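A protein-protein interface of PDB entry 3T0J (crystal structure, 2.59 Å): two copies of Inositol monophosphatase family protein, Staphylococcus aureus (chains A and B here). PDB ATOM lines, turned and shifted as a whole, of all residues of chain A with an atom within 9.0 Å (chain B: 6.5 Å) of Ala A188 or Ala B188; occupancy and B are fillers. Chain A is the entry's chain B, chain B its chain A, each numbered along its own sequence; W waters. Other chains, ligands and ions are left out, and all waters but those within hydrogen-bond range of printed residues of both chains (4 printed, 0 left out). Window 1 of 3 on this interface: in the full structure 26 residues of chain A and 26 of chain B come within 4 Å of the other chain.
Water W1 lies within hydrogen-bond range of the side-chain hydroxyl (OH) of Tyr B189, the backbone carbonyl oxygen (O) of Tyr A189, the side-chain amide oxygen (OE1) of Gln A102 and the side-chain amide nitrogen (ND2) of Asn A98. Water W2 lies within hydrogen-bond range of O of Gly B190 (2.6 Å) and NH2 of Arg A187 (2.8 Å). Water W3 bridges the backbone carbonyl oxygen of Tyr B189 (2.7 Å) and the side-chain hydroxyl of Tyr A189 (2.7 Å). Water W4 lies within hydrogen-bond range of N of Asn A98 (2.7 Å), O of Gly A190 (2.9 Å) and NH2 of Arg B187 (3.1 Å).
Printed residues of chain B within 4 Å of Pro A164: Ile B162 (3.4 Å), Pro B164 (3.5 Å) and Ala B186 (3.6 Å). Of the printed residues of chain B, Ser A185 touches Asn B163. Of chain B, only Arg B187 (3.3 Å), Ala B188 (2.8 Å) and Tyr B189 (3.9 Å) come within 4 Å of Ala A188. Of the printed residues of chain A, Tyr B189 touches Gln A102, Arg A187, Ala A188 and Tyr A189.
Ile A162 touches Pro B164, and with the chains exchanged Pro A164 touches Ile B162. Asn A163 touches Arg B187, and with the chains exchanged Arg A187 touches Asn B163. Pro A164 touches Ala B186, and with the chains exchanged Ala A186 touches Pro B164. Arg A187 touches Gly B190, and with the chains exchanged Gly A190 touches Arg B187. Positions printed for both chains: 160, 161, 162, 163, 164, 186, 187, 188, 189, 190, 191, 195 and 204. Of the 22 pairs that touch across the chains among the printed residues, 19 have their exchanged pair printed and touching as well.
CG of Pro B164 touches O of Ile A162 (3.4 Å). Arg B187 touches Asn A163 (NH1 to ND2, 3.6 Å). Pro A164 touches Ala B186 (CG to CB, 3.6 Å). CB of Ala A186 touches CG of Pro B164, at 3.6 Å. Arg A187 touches Ala B188. CZ of Arg A187 touches CA of Gly B190, 3.6 Å away. Tyr B189 touches Ala A188 (CE1 to O, 3.9 Å). O of Tyr A189 touches NE of Arg B187, 3.5 Å away. Tyr A189 touches Ala B188. Tyr B189 touches Tyr A189 (CD1 to CD1, 3.7 Å).
Of the 25 printed residues of chain A, 11 touch a printed residue of chain B. Hydrophobic or aromatic side chains of chain A that line the printed part of chain B: Pro A164, Ala A186 and Tyr A189. Hydrophobic or aromatic side chains of chain B within 4 Å of the printed part of chain A: Pro B164, Ala B186, Ala B188 and Tyr B189. Among the printed residues, no Asp or Glu carboxylate lies within 4 Å of a Lys or Arg side-chain nitrogen of the other chain.
The backbone NH (N) of Ile B162 sits at hydrogen-bond distance from the backbone carbonyl oxygen (O) of Arg B187, at 2.9 Å. ND2 of Asn A98 sits at hydrogen-bond distance from O of Asn A105 (3.0 Å). The side-chain carboxylate (OE2) of Glu A195 lies within hydrogen-bond range of the backbone NH (N) of Tyr A189, 3.1 Å away. The side-chain amide oxygen of Asn A98 lies close to the side-chain amide oxygen of Gln A102 (3.2 Å). N of Gly B190 sits at hydrogen-bond distance from OE2 of Glu B195 (3.2 Å). ND2 of Asn A105 lies within hydrogen-bond range of OE1 of Gln A102 (3.3 Å).
OD1 of Asn B163 sits close to O of Ala A186, 3.0 Å away. OD1 of Asn A98 is in hydrogen-bond range of NH2 of Arg B187 (3.0 Å). The backbone NH (N) of Ala B188 lies within hydrogen-bond range of the backbone carbonyl oxygen (O) of Ala A188, at 2.8 Å. The side-chain amide nitrogen (ND2) of Asn A163 sits at hydrogen-bond distance from the backbone carbonyl oxygen (O) of Ala B186, at 3.3 Å. NE of Arg A187 sits at hydrogen-bond distance from O of Tyr B189, at 3.2 Å. The side-chain amide nitrogen (NE2) of Gln A102 sits at hydrogen-bond distance from the side-chain hydroxyl (OH) of Tyr B189, at 3.0 Å. OD1 of Asn B163 lies within hydrogen-bond range of OG of Ser A185, at 3.2 Å.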
ATOM      1  N   ASN A  98      20.751   0.667 -20.429  1.00  0.00           N
ATOM      2  CA  ASN A  98      19.680   0.676 -19.445  1.00  0.00           C
ATOM      3  C   ASN A  98      18.310   0.902 -20.076  1.00  0.00           C
ATOM      4  O   ASN A  98      17.369   0.161 -19.794  1.00  0.00           O
ATOM      5  CB  ASN A  98      19.958   1.719 -18.361  1.00  0.00           C
ATOM      6  CG  ASN A  98      21.073   1.294 -17.430  1.00  0.00           C
ATOM      7  OD1 ASN A  98      21.686   0.224 -17.599  1.00  0.00           O
ATOM      8  ND2 ASN A  98      21.351   2.123 -16.447  1.00  0.00           N
ATOM      9  N   GLN A 102      16.344  -2.209 -19.430  1.00  0.00           N
ATOM     10  CA  GLN A 102      15.632  -2.050 -18.180  1.00  0.00           C
ATOM     11  C   GLN A 102      14.426  -1.109 -18.318  1.00  0.00           C
ATOM     12  O   GLN A 102      13.545  -1.087 -17.461  1.00  0.00           O
ATOM     13  CB  GLN A 102      16.597  -1.540 -17.111  1.00  0.00           C
ATOM     14  CG  GLN A 102      17.921  -2.332 -17.061  1.00  0.00           C
ATOM     15  CD  GLN A 102      18.850  -1.875 -15.968  1.00  0.00           C
ATOM     16  OE1 GLN A 102      19.152  -0.698 -15.869  1.00  0.00           O
ATOM     17  NE2 GLN A 102      19.318  -2.811 -15.135  1.00  0.00           N
ATOM     18  N   ASN A 105      16.357   3.806 -15.348  1.00  0.00           N
ATOM     19  CA  ASN A 105      17.724   4.133 -14.915  1.00  0.00           C
ATOM     20  C   ASN A 105      18.532   4.865 -15.995  1.00  0.00           C
ATOM     21  O   ASN A 105      19.739   4.599 -16.186  1.00  0.00           O
ATOM     22  CB  ASN A 105      18.495   2.870 -14.466  1.00  0.00           C
ATOM     23  CG  ASN A 105      17.874   2.174 -13.251  1.00  0.00           C
ATOM     24  OD1 ASN A 105      17.404   2.819 -12.309  1.00  0.00           O
ATOM     25  ND2 ASN A 105      17.911   0.850 -13.256  1.00  0.00           N
ATOM     26  N   ILE A 159      32.616   4.273  -0.982  1.00  0.00           N
ATOM     27  CA  ILE A 159      32.119   3.428  -2.071  1.00  0.00           C
ATOM     28  C   ILE A 159      32.336   4.175  -3.347  1.00  0.00           C
ATOM     29  O   ILE A 159      32.130   5.398  -3.406  1.00  0.00           O
ATOM     30  CB  ILE A 159      30.658   3.083  -1.956  1.00  0.00           C
ATOM     31  CG1 ILE A 159      30.380   2.418  -0.623  1.00  0.00           C
ATOM     32  CG2 ILE A 159      30.308   2.124  -3.057  1.00  0.00           C
ATOM     33  CD1 ILE A 159      29.074   1.677  -0.601  1.00  0.00           C
ATOM     34  N   ILE A 160      32.773   3.468  -4.366  1.00  0.00           N
ATOM     35  CA  ILE A 160      33.120   4.137  -5.581  1.00  0.00           C
ATOM     36  C   ILE A 160      32.307   3.520  -6.707  1.00  0.00           C
ATOM     37  O   ILE A 160      31.978   2.313  -6.642  1.00  0.00           O
ATOM     38  CB  ILE A 160      34.610   3.954  -5.915  1.00  0.00           C
ATOM     39  CG1 ILE A 160      34.924   2.466  -6.039  1.00  0.00           C
ATOM     40  CG2 ILE A 160      35.478   4.610  -4.888  1.00  0.00           C
ATOM     41  CD1 ILE A 160      36.127   2.143  -6.904  1.00  0.00           C
ATOM     42  N   GLY A 161      32.007   4.329  -7.734  1.00  0.00           N
ATOM     43  CA  GLY A 161      31.421   3.821  -8.959  1.00  0.00           C
ATOM     44  C   GLY A 161      32.430   3.632 -10.065  1.00  0.00           C
ATOM     45  O   GLY A 161      33.195   4.540 -10.397  1.00  0.00           O
ATOM     46  N   ILE A 162      32.445   2.431 -10.630  1.00  0.00           N
ATOM     47  CA  ILE A 162      33.327   2.110 -11.744  1.00  0.00           C
ATOM     48  C   ILE A 162      32.848   0.838 -12.440  1.00  0.00           C
ATOM     49  O   ILE A 162      32.679  -0.190 -11.794  1.00  0.00           O
ATOM     50  CB  ILE A 162      34.821   1.960 -11.298  1.00  0.00           C
ATOM     51  CG1 ILE A 162      35.718   1.733 -12.534  1.00  0.00           C
ATOM     52  CG2 ILE A 162      34.966   0.878 -10.243  1.00  0.00           C
ATOM     53  CD1 ILE A 162      37.211   1.687 -12.259  1.00  0.00           C
ATOM     54  N   ASN A 163      32.655   0.901 -13.757  1.00  0.00           N
ATOM     55  CA  ASN A 163      32.132  -0.235 -14.465  1.00  0.00           C
ATOM     56  C   ASN A 163      33.152  -1.368 -14.401  1.00  0.00           C
ATOM     57  O   ASN A 163      34.352  -1.147 -14.467  1.00  0.00           O
ATOM     58  CB  ASN A 163      31.804   0.149 -15.890  1.00  0.00           C
ATOM     59  CG  ASN A 163      31.008  -0.935 -16.639  1.00  0.00           C
ATOM     60  OD1 ASN A 163      31.482  -2.055 -16.850  1.00  0.00           O
ATOM     61  ND2 ASN A 163      29.819  -0.586 -17.073  1.00  0.00           N
ATOM     62  N   PRO A 164      32.686  -2.597 -14.229  1.00  0.00           N
ATOM     63  CA  PRO A 164      33.659  -3.696 -14.179  1.00  0.00           C
ATOM     64  C   PRO A 164      34.444  -3.831 -15.461  1.00  0.00           C
ATOM     65  O   PRO A 164      35.552  -4.417 -15.490  1.00  0.00           O
ATOM     66  CB  PRO A 164      32.777  -4.908 -13.991  1.00  0.00           C
ATOM     67  CG  PRO A 164      31.677  -4.388 -13.168  1.00  0.00           C
ATOM     68  CD  PRO A 164      31.393  -2.987 -13.654  1.00  0.00           C
ATOM     69  N   ASN A 165      33.875  -3.282 -16.521  1.00  0.00           N
ATOM     70  CA  ASN A 165      34.430  -3.486 -17.827  1.00  0.00           C
ATOM     71  C   ASN A 165      35.835  -2.909 -17.944  1.00  0.00           C
ATOM     72  O   ASN A 165      36.696  -3.466 -18.608  1.00  0.00           O
ATOM     73  CB  ASN A 165      33.495  -2.909 -18.874  1.00  0.00           C
ATOM     74  CG  ASN A 165      33.353  -3.820 -20.039  1.00  0.00           C
ATOM     75  OD1 ASN A 165      34.085  -3.720 -21.021  1.00  0.00           O
ATOM     76  ND2 ASN A 165      32.444  -4.765 -19.917  1.00  0.00           N
ATOM     77  N   TRP A 166      36.068  -1.805 -17.250  1.00  0.00           N
ATOM     78  CA  TRP A 166      37.344  -1.128 -17.311  1.00  0.00           C
ATOM     79  C   TRP A 166      38.455  -1.961 -16.682  1.00  0.00           C
ATOM     80  O   TRP A 166      39.638  -1.752 -16.952  1.00  0.00           O
ATOM     81  CB  TRP A 166      37.243   0.249 -16.651  1.00  0.00           C
ATOM     82  CG  TRP A 166      36.219   1.158 -17.246  1.00  0.00           C
ATOM     83  CD1 TRP A 166      35.246   1.855 -16.563  1.00  0.00           C
ATOM     84  CD2 TRP A 166      36.043   1.487 -18.627  1.00  0.00           C
ATOM     85  NE1 TRP A 166      34.494   2.593 -17.424  1.00  0.00           N
ATOM     86  CE2 TRP A 166      34.951   2.385 -18.704  1.00  0.00           C
ATOM     87  CE3 TRP A 166      36.696   1.111 -19.811  1.00  0.00           C
ATOM     88  CZ2 TRP A 166      34.491   2.910 -19.920  1.00  0.00           C
ATOM     89  CZ3 TRP A 166      36.250   1.646 -21.021  1.00  0.00           C
ATOM     90  CH2 TRP A 166      35.144   2.527 -21.061  1.00  0.00           C
ATOM     91  N   SER A 185      33.891  -0.704  -1.158  1.00  0.00           N
ATOM     92  CA  SER A 185      33.215  -1.516  -2.152  1.00  0.00           C
ATOM     93  C   SER A 185      32.970  -0.701  -3.446  1.00  0.00           C
ATOM     94  O   SER A 185      33.403   0.447  -3.570  1.00  0.00           O
ATOM     95  CB  SER A 185      31.907  -2.115  -1.608  1.00  0.00           C
ATOM     96  OG  SER A 185      31.234  -2.885  -2.624  1.00  0.00           O
ATOM     97  N   ALA A 186      32.304  -1.308  -4.422  1.00  0.00           N
ATOM     98  CA  ALA A 186      32.116  -0.639  -5.677  1.00  0.00           C
ATOM     99  C   ALA A 186      30.750  -0.914  -6.226  1.00  0.00           C
ATOM    100  O   ALA A 186      30.154  -1.944  -5.938  1.00  0.00           O
ATOM    101  CB  ALA A 186      33.175  -1.063  -6.672  1.00  0.00           C
ATOM    102  N   ARG A 187      30.265   0.041  -7.007  1.00  0.00           N
ATOM    103  CA  ARG A 187      29.006  -0.055  -7.671  1.00  0.00           C
ATOM    104  C   ARG A 187      29.161   0.412  -9.136  1.00  0.00           C
ATOM    105  O   ARG A 187      30.102   1.177  -9.457  1.00  0.00           O
ATOM    106  CB  ARG A 187      28.005   0.840  -6.961  1.00  0.00           C
ATOM    107  CG  ARG A 187      27.850   0.622  -5.478  1.00  0.00           C
ATOM    108  CD  ARG A 187      26.984  -0.580  -5.197  1.00  0.00           C
ATOM    109  NE  ARG A 187      26.759  -0.774  -3.777  1.00  0.00           N
ATOM    110  CZ  ARG A 187      27.557  -1.485  -2.978  1.00  0.00           C
ATOM    111  NH1 ARG A 187      28.669  -2.061  -3.453  1.00  0.00           N
ATOM    112  NH2 ARG A 187      27.233  -1.589  -1.684  1.00  0.00           N
ATOM    113  N   ALA A 188      28.227  -0.016 -10.005  1.00  0.00           N
ATOM    114  CA  ALA A 188      28.104   0.538 -11.339  1.00  0.00           C
ATOM    115  C   ALA A 188      26.657   0.519 -11.811  1.00  0.00           C
ATOM    116  O   ALA A 188      25.976  -0.500 -11.713  1.00  0.00           O
ATOM    117  CB  ALA A 188      29.002  -0.219 -12.320  1.00  0.00           C
ATOM    118  N   TYR A 189      26.235   1.634 -12.402  1.00  0.00           N
ATOM    119  CA  TYR A 189      24.832   1.928 -12.665  1.00  0.00           C
ATOM    120  C   TYR A 189      24.506   2.114 -14.128  1.00  0.00           C
ATOM    121  O   TYR A 189      23.333   2.018 -14.502  1.00  0.00           O
ATOM    122  CB  TYR A 189      24.388   3.174 -11.878  1.00  0.00           C
ATOM    123  CG  TYR A 189      24.465   2.958 -10.389  1.00  0.00           C
ATOM    124  CD1 TYR A 189      23.897   1.826  -9.798  1.00  0.00           C
ATOM    125  CD2 TYR A 189      25.135   3.855  -9.564  1.00  0.00           C
ATOM    126  CE1 TYR A 189      23.994   1.617  -8.439  1.00  0.00           C
ATOM    127  CE2 TYR A 189      25.218   3.647  -8.201  1.00  0.00           C
ATOM    128  CZ  TYR A 189      24.648   2.537  -7.651  1.00  0.00           C
ATOM    129  OH  TYR A 189      24.709   2.346  -6.292  1.00  0.00           O
ATOM    130  N   GLY A 190      25.519   2.384 -14.953  1.00  0.00           N
ATOM    131  CA  GLY A 190      25.327   2.380 -16.418  1.00  0.00           C
ATOM    132  C   GLY A 190      24.897   3.725 -16.994  1.00  0.00           C
ATOM    133  O   GLY A 190      24.581   3.798 -18.177  1.00  0.00           O
ATOM    134  N   SER A 191      24.895   4.783 -16.157  1.00  0.00           N
ATOM    135  CA  SER A 191      24.613   6.127 -16.606  1.00  0.00           C
ATOM    136  C   SER A 191      25.545   7.145 -15.955  1.00  0.00           C
ATOM    137  O   SER A 191      25.341   7.546 -14.781  1.00  0.00           O
ATOM    138  CB  SER A 191      23.189   6.502 -16.252  1.00  0.00           C
ATOM    139  OG  SER A 191      22.969   7.878 -16.518  1.00  0.00           O
ATOM    140  N   ALA A 192      26.555   7.596 -16.697  1.00  0.00           N
ATOM    141  CA  ALA A 192      27.536   8.463 -16.074  1.00  0.00           C
ATOM    142  C   ALA A 192      26.934   9.728 -15.418  1.00  0.00           C
ATOM    143  O   ALA A 192      27.367  10.123 -14.299  1.00  0.00           O
ATOM    144  CB  ALA A 192      28.620   8.809 -17.038  1.00  0.00           C
ATOM    145  N   GLU A 195      25.556   8.841 -12.128  1.00  0.00           N
ATOM    146  CA  GLU A 195      26.618   8.392 -11.206  1.00  0.00           C
ATOM    147  C   GLU A 195      27.306   9.623 -10.653  1.00  0.00           C
ATOM    148  O   GLU A 195      27.644   9.667  -9.486  1.00  0.00           O
ATOM    149  CB  GLU A 195      27.619   7.440 -11.891  1.00  0.00           C
ATOM    150  CG  GLU A 195      27.122   5.982 -12.038  1.00  0.00           C
ATOM    151  CD  GLU A 195      27.716   5.211 -13.236  1.00  0.00           C
ATOM    152  OE1 GLU A 195      27.829   5.774 -14.364  1.00  0.00           O
ATOM    153  OE2 GLU A 195      28.070   4.018 -13.044  1.00  0.00           O
ATOM    154  N   SER A 198      25.096  10.684  -8.298  1.00  0.00           N
ATOM    155  CA  SER A 198      25.261   9.907  -7.060  1.00  0.00           C
ATOM    156  C   SER A 198      26.323  10.441  -6.089  1.00  0.00           C
ATOM    157  O   SER A 198      26.104  10.429  -4.874  1.00  0.00           O
ATOM    158  CB  SER A 198      25.477   8.465  -7.379  1.00  0.00           C
ATOM    159  OG  SER A 198      24.221   8.013  -7.768  1.00  0.00           O
ATOM    160  N   LEU A 204      27.347   7.736  -3.808  1.00  0.00           N
ATOM    161  CA  LEU A 204      28.713   7.284  -4.026  1.00  0.00           C
ATOM    162  C   LEU A 204      29.653   8.352  -3.430  1.00  0.00           C
ATOM    163  O   LEU A 204      29.300   9.537  -3.431  1.00  0.00           O
ATOM    164  CB  LEU A 204      28.998   7.094  -5.525  1.00  0.00           C
ATOM    165  CG  LEU A 204      28.082   6.061  -6.152  1.00  0.00           C
ATOM    166  CD1 LEU A 204      28.305   5.914  -7.626  1.00  0.00           C
ATOM    167  CD2 LEU A 204      28.326   4.758  -5.432  1.00  0.00           C
ATOM    168  N   ALA A 206      32.881   8.420  -4.662  1.00  0.00           N
ATOM    169  CA  ALA A 206      33.553   8.750  -5.909  1.00  0.00           C
ATOM    170  C   ALA A 206      33.042   7.945  -7.113  1.00  0.00           C
ATOM    171  O   ALA A 206      32.360   6.909  -6.986  1.00  0.00           O
ATOM    172  CB  ALA A 206      35.064   8.602  -5.770  1.00  0.00           C
ATOM    173  N   TYR A 207      33.394   8.435  -8.291  1.00  0.00           N
ATOM    174  CA  TYR A 207      33.030   7.781  -9.524  1.00  0.00           C
ATOM    175  C   TYR A 207      34.158   8.042 -10.487  1.00  0.00           C
ATOM    176  O   TYR A 207      34.720   9.132 -10.480  1.00  0.00           O
ATOM    177  CB  TYR A 207      31.726   8.363 -10.078  1.00  0.00           C
ATOM    178  CG  TYR A 207      31.432   7.928 -11.496  1.00  0.00           C
ATOM    179  CD1 TYR A 207      31.083   6.608 -11.781  1.00  0.00           C
ATOM    180  CD2 TYR A 207      31.488   8.830 -12.551  1.00  0.00           C
ATOM    181  CE1 TYR A 207      30.815   6.201 -13.086  1.00  0.00           C
ATOM    182  CE2 TYR A 207      31.198   8.419 -13.889  1.00  0.00           C
ATOM    183  CZ  TYR A 207      30.867   7.109 -14.125  1.00  0.00           C
ATOM    184  OH  TYR A 207      30.611   6.674 -15.396  1.00  0.00           O
ATOM    185  N   MET A 208      34.488   7.061 -11.320  1.00  0.00           N
ATOM    186  CA  MET A 208      35.555   7.255 -12.301  1.00  0.00           C
ATOM    187  C   MET A 208      35.305   6.505 -13.596  1.00  0.00           C
ATOM    188  O   MET A 208      34.584   5.499 -13.622  1.00  0.00           O
ATOM    189  CB  MET A 208      36.923   6.874 -11.722  1.00  0.00           C
ATOM    190  CG  MET A 208      37.096   5.441 -11.312  1.00  0.00           C
ATOM    191  SD  MET A 208      38.183   5.406  -9.853  1.00  0.00           S
ATOM    192  CE  MET A 208      36.987   5.755  -8.586  1.00  0.00           C
ATOM    193  N   ILE B 160      25.195  -8.182 -17.337  1.00  0.00           N
ATOM    194  CA  ILE B 160      25.339  -9.044 -16.164  1.00  0.00           C
ATOM    195  C   ILE B 160      25.645  -8.225 -14.894  1.00  0.00           C
ATOM    196  O   ILE B 160      26.217  -7.142 -14.965  1.00  0.00           O
ATOM    197  CB  ILE B 160      26.421 -10.103 -16.417  1.00  0.00           C
ATOM    198  CG1 ILE B 160      27.786  -9.423 -16.613  1.00  0.00           C
ATOM    199  CG2 ILE B 160      26.068 -10.911 -17.659  1.00  0.00           C
ATOM    200  CD1 ILE B 160      28.971 -10.349 -16.579  1.00  0.00           C
ATOM    201  N   GLY B 161      25.248  -8.733 -13.738  1.00  0.00           N
ATOM    202  CA  GLY B 161      25.551  -8.055 -12.500  1.00  0.00           C
ATOM    203  C   GLY B 161      26.747  -8.727 -11.873  1.00  0.00           C
ATOM    204  O   GLY B 161      26.767  -9.960 -11.732  1.00  0.00           O
ATOM    205  N   ILE B 162      27.742  -7.938 -11.504  1.00  0.00           N
ATOM    206  CA  ILE B 162      28.963  -8.455 -10.887  1.00  0.00           C
ATOM    207  C   ILE B 162      29.765  -7.342 -10.198  1.00  0.00           C
ATOM    208  O   ILE B 162      30.145  -6.388 -10.869  1.00  0.00           O
ATOM    209  CB  ILE B 162      29.877  -9.089 -11.951  1.00  0.00           C
ATOM    210  CG1 ILE B 162      31.241  -9.416 -11.356  1.00  0.00           C
ATOM    211  CG2 ILE B 162      30.089  -8.149 -13.132  1.00  0.00           C
ATOM    212  CD1 ILE B 162      31.759 -10.729 -11.900  1.00  0.00           C
ATOM    213  N   ASN B 163      30.063  -7.450  -8.901  1.00  0.00           N
ATOM    214  CA  ASN B 163      30.847  -6.391  -8.248  1.00  0.00           C
ATOM    215  C   ASN B 163      32.263  -6.341  -8.792  1.00  0.00           C
ATOM    216  O   ASN B 163      32.947  -7.366  -8.845  1.00  0.00           O
ATOM    217  CB  ASN B 163      30.881  -6.562  -6.754  1.00  0.00           C
ATOM    218  CG  ASN B 163      31.439  -5.334  -6.026  1.00  0.00           C
ATOM    219  OD1 ASN B 163      30.788  -4.788  -5.141  1.00  0.00           O
ATOM    220  ND2 ASN B 163      32.644  -4.920  -6.362  1.00  0.00           N
ATOM    221  N   PRO B 164      32.706  -5.157  -9.227  1.00  0.00           N
ATOM    222  CA  PRO B 164      34.082  -4.924  -9.638  1.00  0.00           C
ATOM    223  C   PRO B 164      35.159  -5.515  -8.736  1.00  0.00           C
ATOM    224  O   PRO B 164      36.225  -5.850  -9.219  1.00  0.00           O
ATOM    225  CB  PRO B 164      34.196  -3.388  -9.629  1.00  0.00           C
ATOM    226  CG  PRO B 164      32.754  -2.877  -9.754  1.00  0.00           C
ATOM    227  CD  PRO B 164      31.827  -4.060  -9.647  1.00  0.00           C
ATOM    228  N   ALA B 186      28.153  -4.367 -17.704  1.00  0.00           N
ATOM    229  CA  ALA B 186      28.077  -4.842 -16.328  1.00  0.00           C
ATOM    230  C   ALA B 186      27.521  -3.808 -15.373  1.00  0.00           C
ATOM    231  O   ALA B 186      27.727  -2.638 -15.551  1.00  0.00           O
ATOM    232  CB  ALA B 186      29.436  -5.293 -15.849  1.00  0.00           C
ATOM    233  N   ARG B 187      26.828  -4.276 -14.344  1.00  0.00           N
ATOM    234  CA  ARG B 187      26.289  -3.409 -13.342  1.00  0.00           C
ATOM    235  C   ARG B 187      26.576  -3.987 -11.966  1.00  0.00           C
ATOM    236  O   ARG B 187      26.838  -5.193 -11.835  1.00  0.00           O
ATOM    237  CB  ARG B 187      24.794  -3.358 -13.518  1.00  0.00           C
ATOM    238  CG  ARG B 187      24.362  -2.857 -14.836  1.00  0.00           C
ATOM    239  CD  ARG B 187      24.611  -1.384 -14.980  1.00  0.00           C
ATOM    240  NE  ARG B 187      24.180  -0.920 -16.286  1.00  0.00           N
ATOM    241  CZ  ARG B 187      24.961  -0.816 -17.348  1.00  0.00           C
ATOM    242  NH1 ARG B 187      26.239  -1.152 -17.261  1.00  0.00           N
ATOM    243  NH2 ARG B 187      24.457  -0.363 -18.502  1.00  0.00           N
ATOM    244  N   ALA B 188      26.465  -3.160 -10.931  1.00  0.00           N
ATOM    245  CA  ALA B 188      26.630  -3.680  -9.601  1.00  0.00           C
ATOM    246  C   ALA B 188      25.896  -2.823  -8.632  1.00  0.00           C
ATOM    247  O   ALA B 188      26.225  -1.638  -8.464  1.00  0.00           O
ATOM    248  CB  ALA B 188      28.087  -3.723  -9.231  1.00  0.00           C
ATOM    249  N   TYR B 189      24.932  -3.436  -7.952  1.00  0.00           N
ATOM    250  CA  TYR B 189      24.010  -2.684  -7.109  1.00  0.00           C
ATOM    251  C   TYR B 189      24.282  -2.840  -5.622  1.00  0.00           C
ATOM    252  O   TYR B 189      23.961  -1.917  -4.833  1.00  0.00           O
ATOM    253  CB  TYR B 189      22.543  -2.985  -7.474  1.00  0.00           C
ATOM    254  CG  TYR B 189      22.223  -2.794  -8.955  1.00  0.00           C
ATOM    255  CD1 TYR B 189      22.503  -1.566  -9.601  1.00  0.00           C
ATOM    256  CD2 TYR B 189      21.647  -3.829  -9.715  1.00  0.00           C
ATOM    257  CE1 TYR B 189      22.221  -1.362 -10.941  1.00  0.00           C
ATOM    258  CE2 TYR B 189      21.345  -3.638 -11.096  1.00  0.00           C
ATOM    259  CZ  TYR B 189      21.645  -2.401 -11.690  1.00  0.00           C
ATOM    260  OH  TYR B 189      21.364  -2.174 -13.023  1.00  0.00           O
ATOM    261  N   GLY B 190      24.885  -3.972  -5.225  1.00  0.00           N
ATOM    262  CA  GLY B 190      25.294  -4.119  -3.846  1.00  0.00           C
ATOM    263  C   GLY B 190      24.220  -4.560  -2.854  1.00  0.00           C
ATOM    264  O   GLY B 190      24.368  -4.318  -1.651  1.00  0.00           O
ATOM    265  N   SER B 191      23.148  -5.190  -3.341  1.00  0.00           N
ATOM    266  CA  SER B 191      22.230  -6.021  -2.517  1.00  0.00           C
ATOM    267  C   SER B 191      21.907  -7.288  -3.315  1.00  0.00           C
ATOM    268  O   SER B 191      21.026  -7.276  -4.173  1.00  0.00           O
ATOM    269  CB  SER B 191      20.913  -5.282  -2.149  1.00  0.00           C
ATOM    270  OG  SER B 191      19.820  -6.183  -1.889  1.00  0.00           O
ATOM    271  N   GLU B 195      19.654  -8.012  -6.475  1.00  0.00           N
ATOM    272  CA  GLU B 195      20.281  -8.351  -7.726  1.00  0.00           C
ATOM    273  C   GLU B 195      19.667  -9.638  -8.330  1.00  0.00           C
ATOM    274  O   GLU B 195      19.483  -9.748  -9.552  1.00  0.00           O
ATOM    275  CB  GLU B 195      21.811  -8.389  -7.577  1.00  0.00           C
ATOM    276  CG  GLU B 195      22.432  -6.971  -7.688  1.00  0.00           C
ATOM    277  CD  GLU B 195      23.773  -6.823  -6.963  1.00  0.00           C
ATOM    278  OE1 GLU B 195      23.879  -7.323  -5.824  1.00  0.00           O
ATOM    279  OE2 GLU B 195      24.711  -6.189  -7.532  1.00  0.00           O
ATOM    280  N   LEU B 204      18.528  -7.415 -15.276  1.00  0.00           N
ATOM    281  CA  LEU B 204      19.862  -7.920 -15.518  1.00  0.00           C
ATOM    282  C   LEU B 204      19.691  -9.286 -16.157  1.00  0.00           C
ATOM    283  O   LEU B 204      18.948 -10.096 -15.617  1.00  0.00           O
ATOM    284  CB  LEU B 204      20.577  -8.117 -14.194  1.00  0.00           C
ATOM    285  CG  LEU B 204      21.173  -6.895 -13.549  1.00  0.00           C
ATOM    286  CD1 LEU B 204      21.806  -7.322 -12.241  1.00  0.00           C
ATOM    287  CD2 LEU B 204      22.196  -6.308 -14.494  1.00  0.00           C
HETATM  288  O   HOH W   1      21.350   0.189 -13.813  1.00  0.00           O
HETATM  289  O   HOH W   2      25.579  -2.845   0.164  1.00  0.00           O
HETATM  290  O   HOH W   3      23.106   0.627  -4.890  1.00  0.00           O
HETATM  291  O   HOH W   4      23.008   2.076 -19.833  1.00  0.00           O
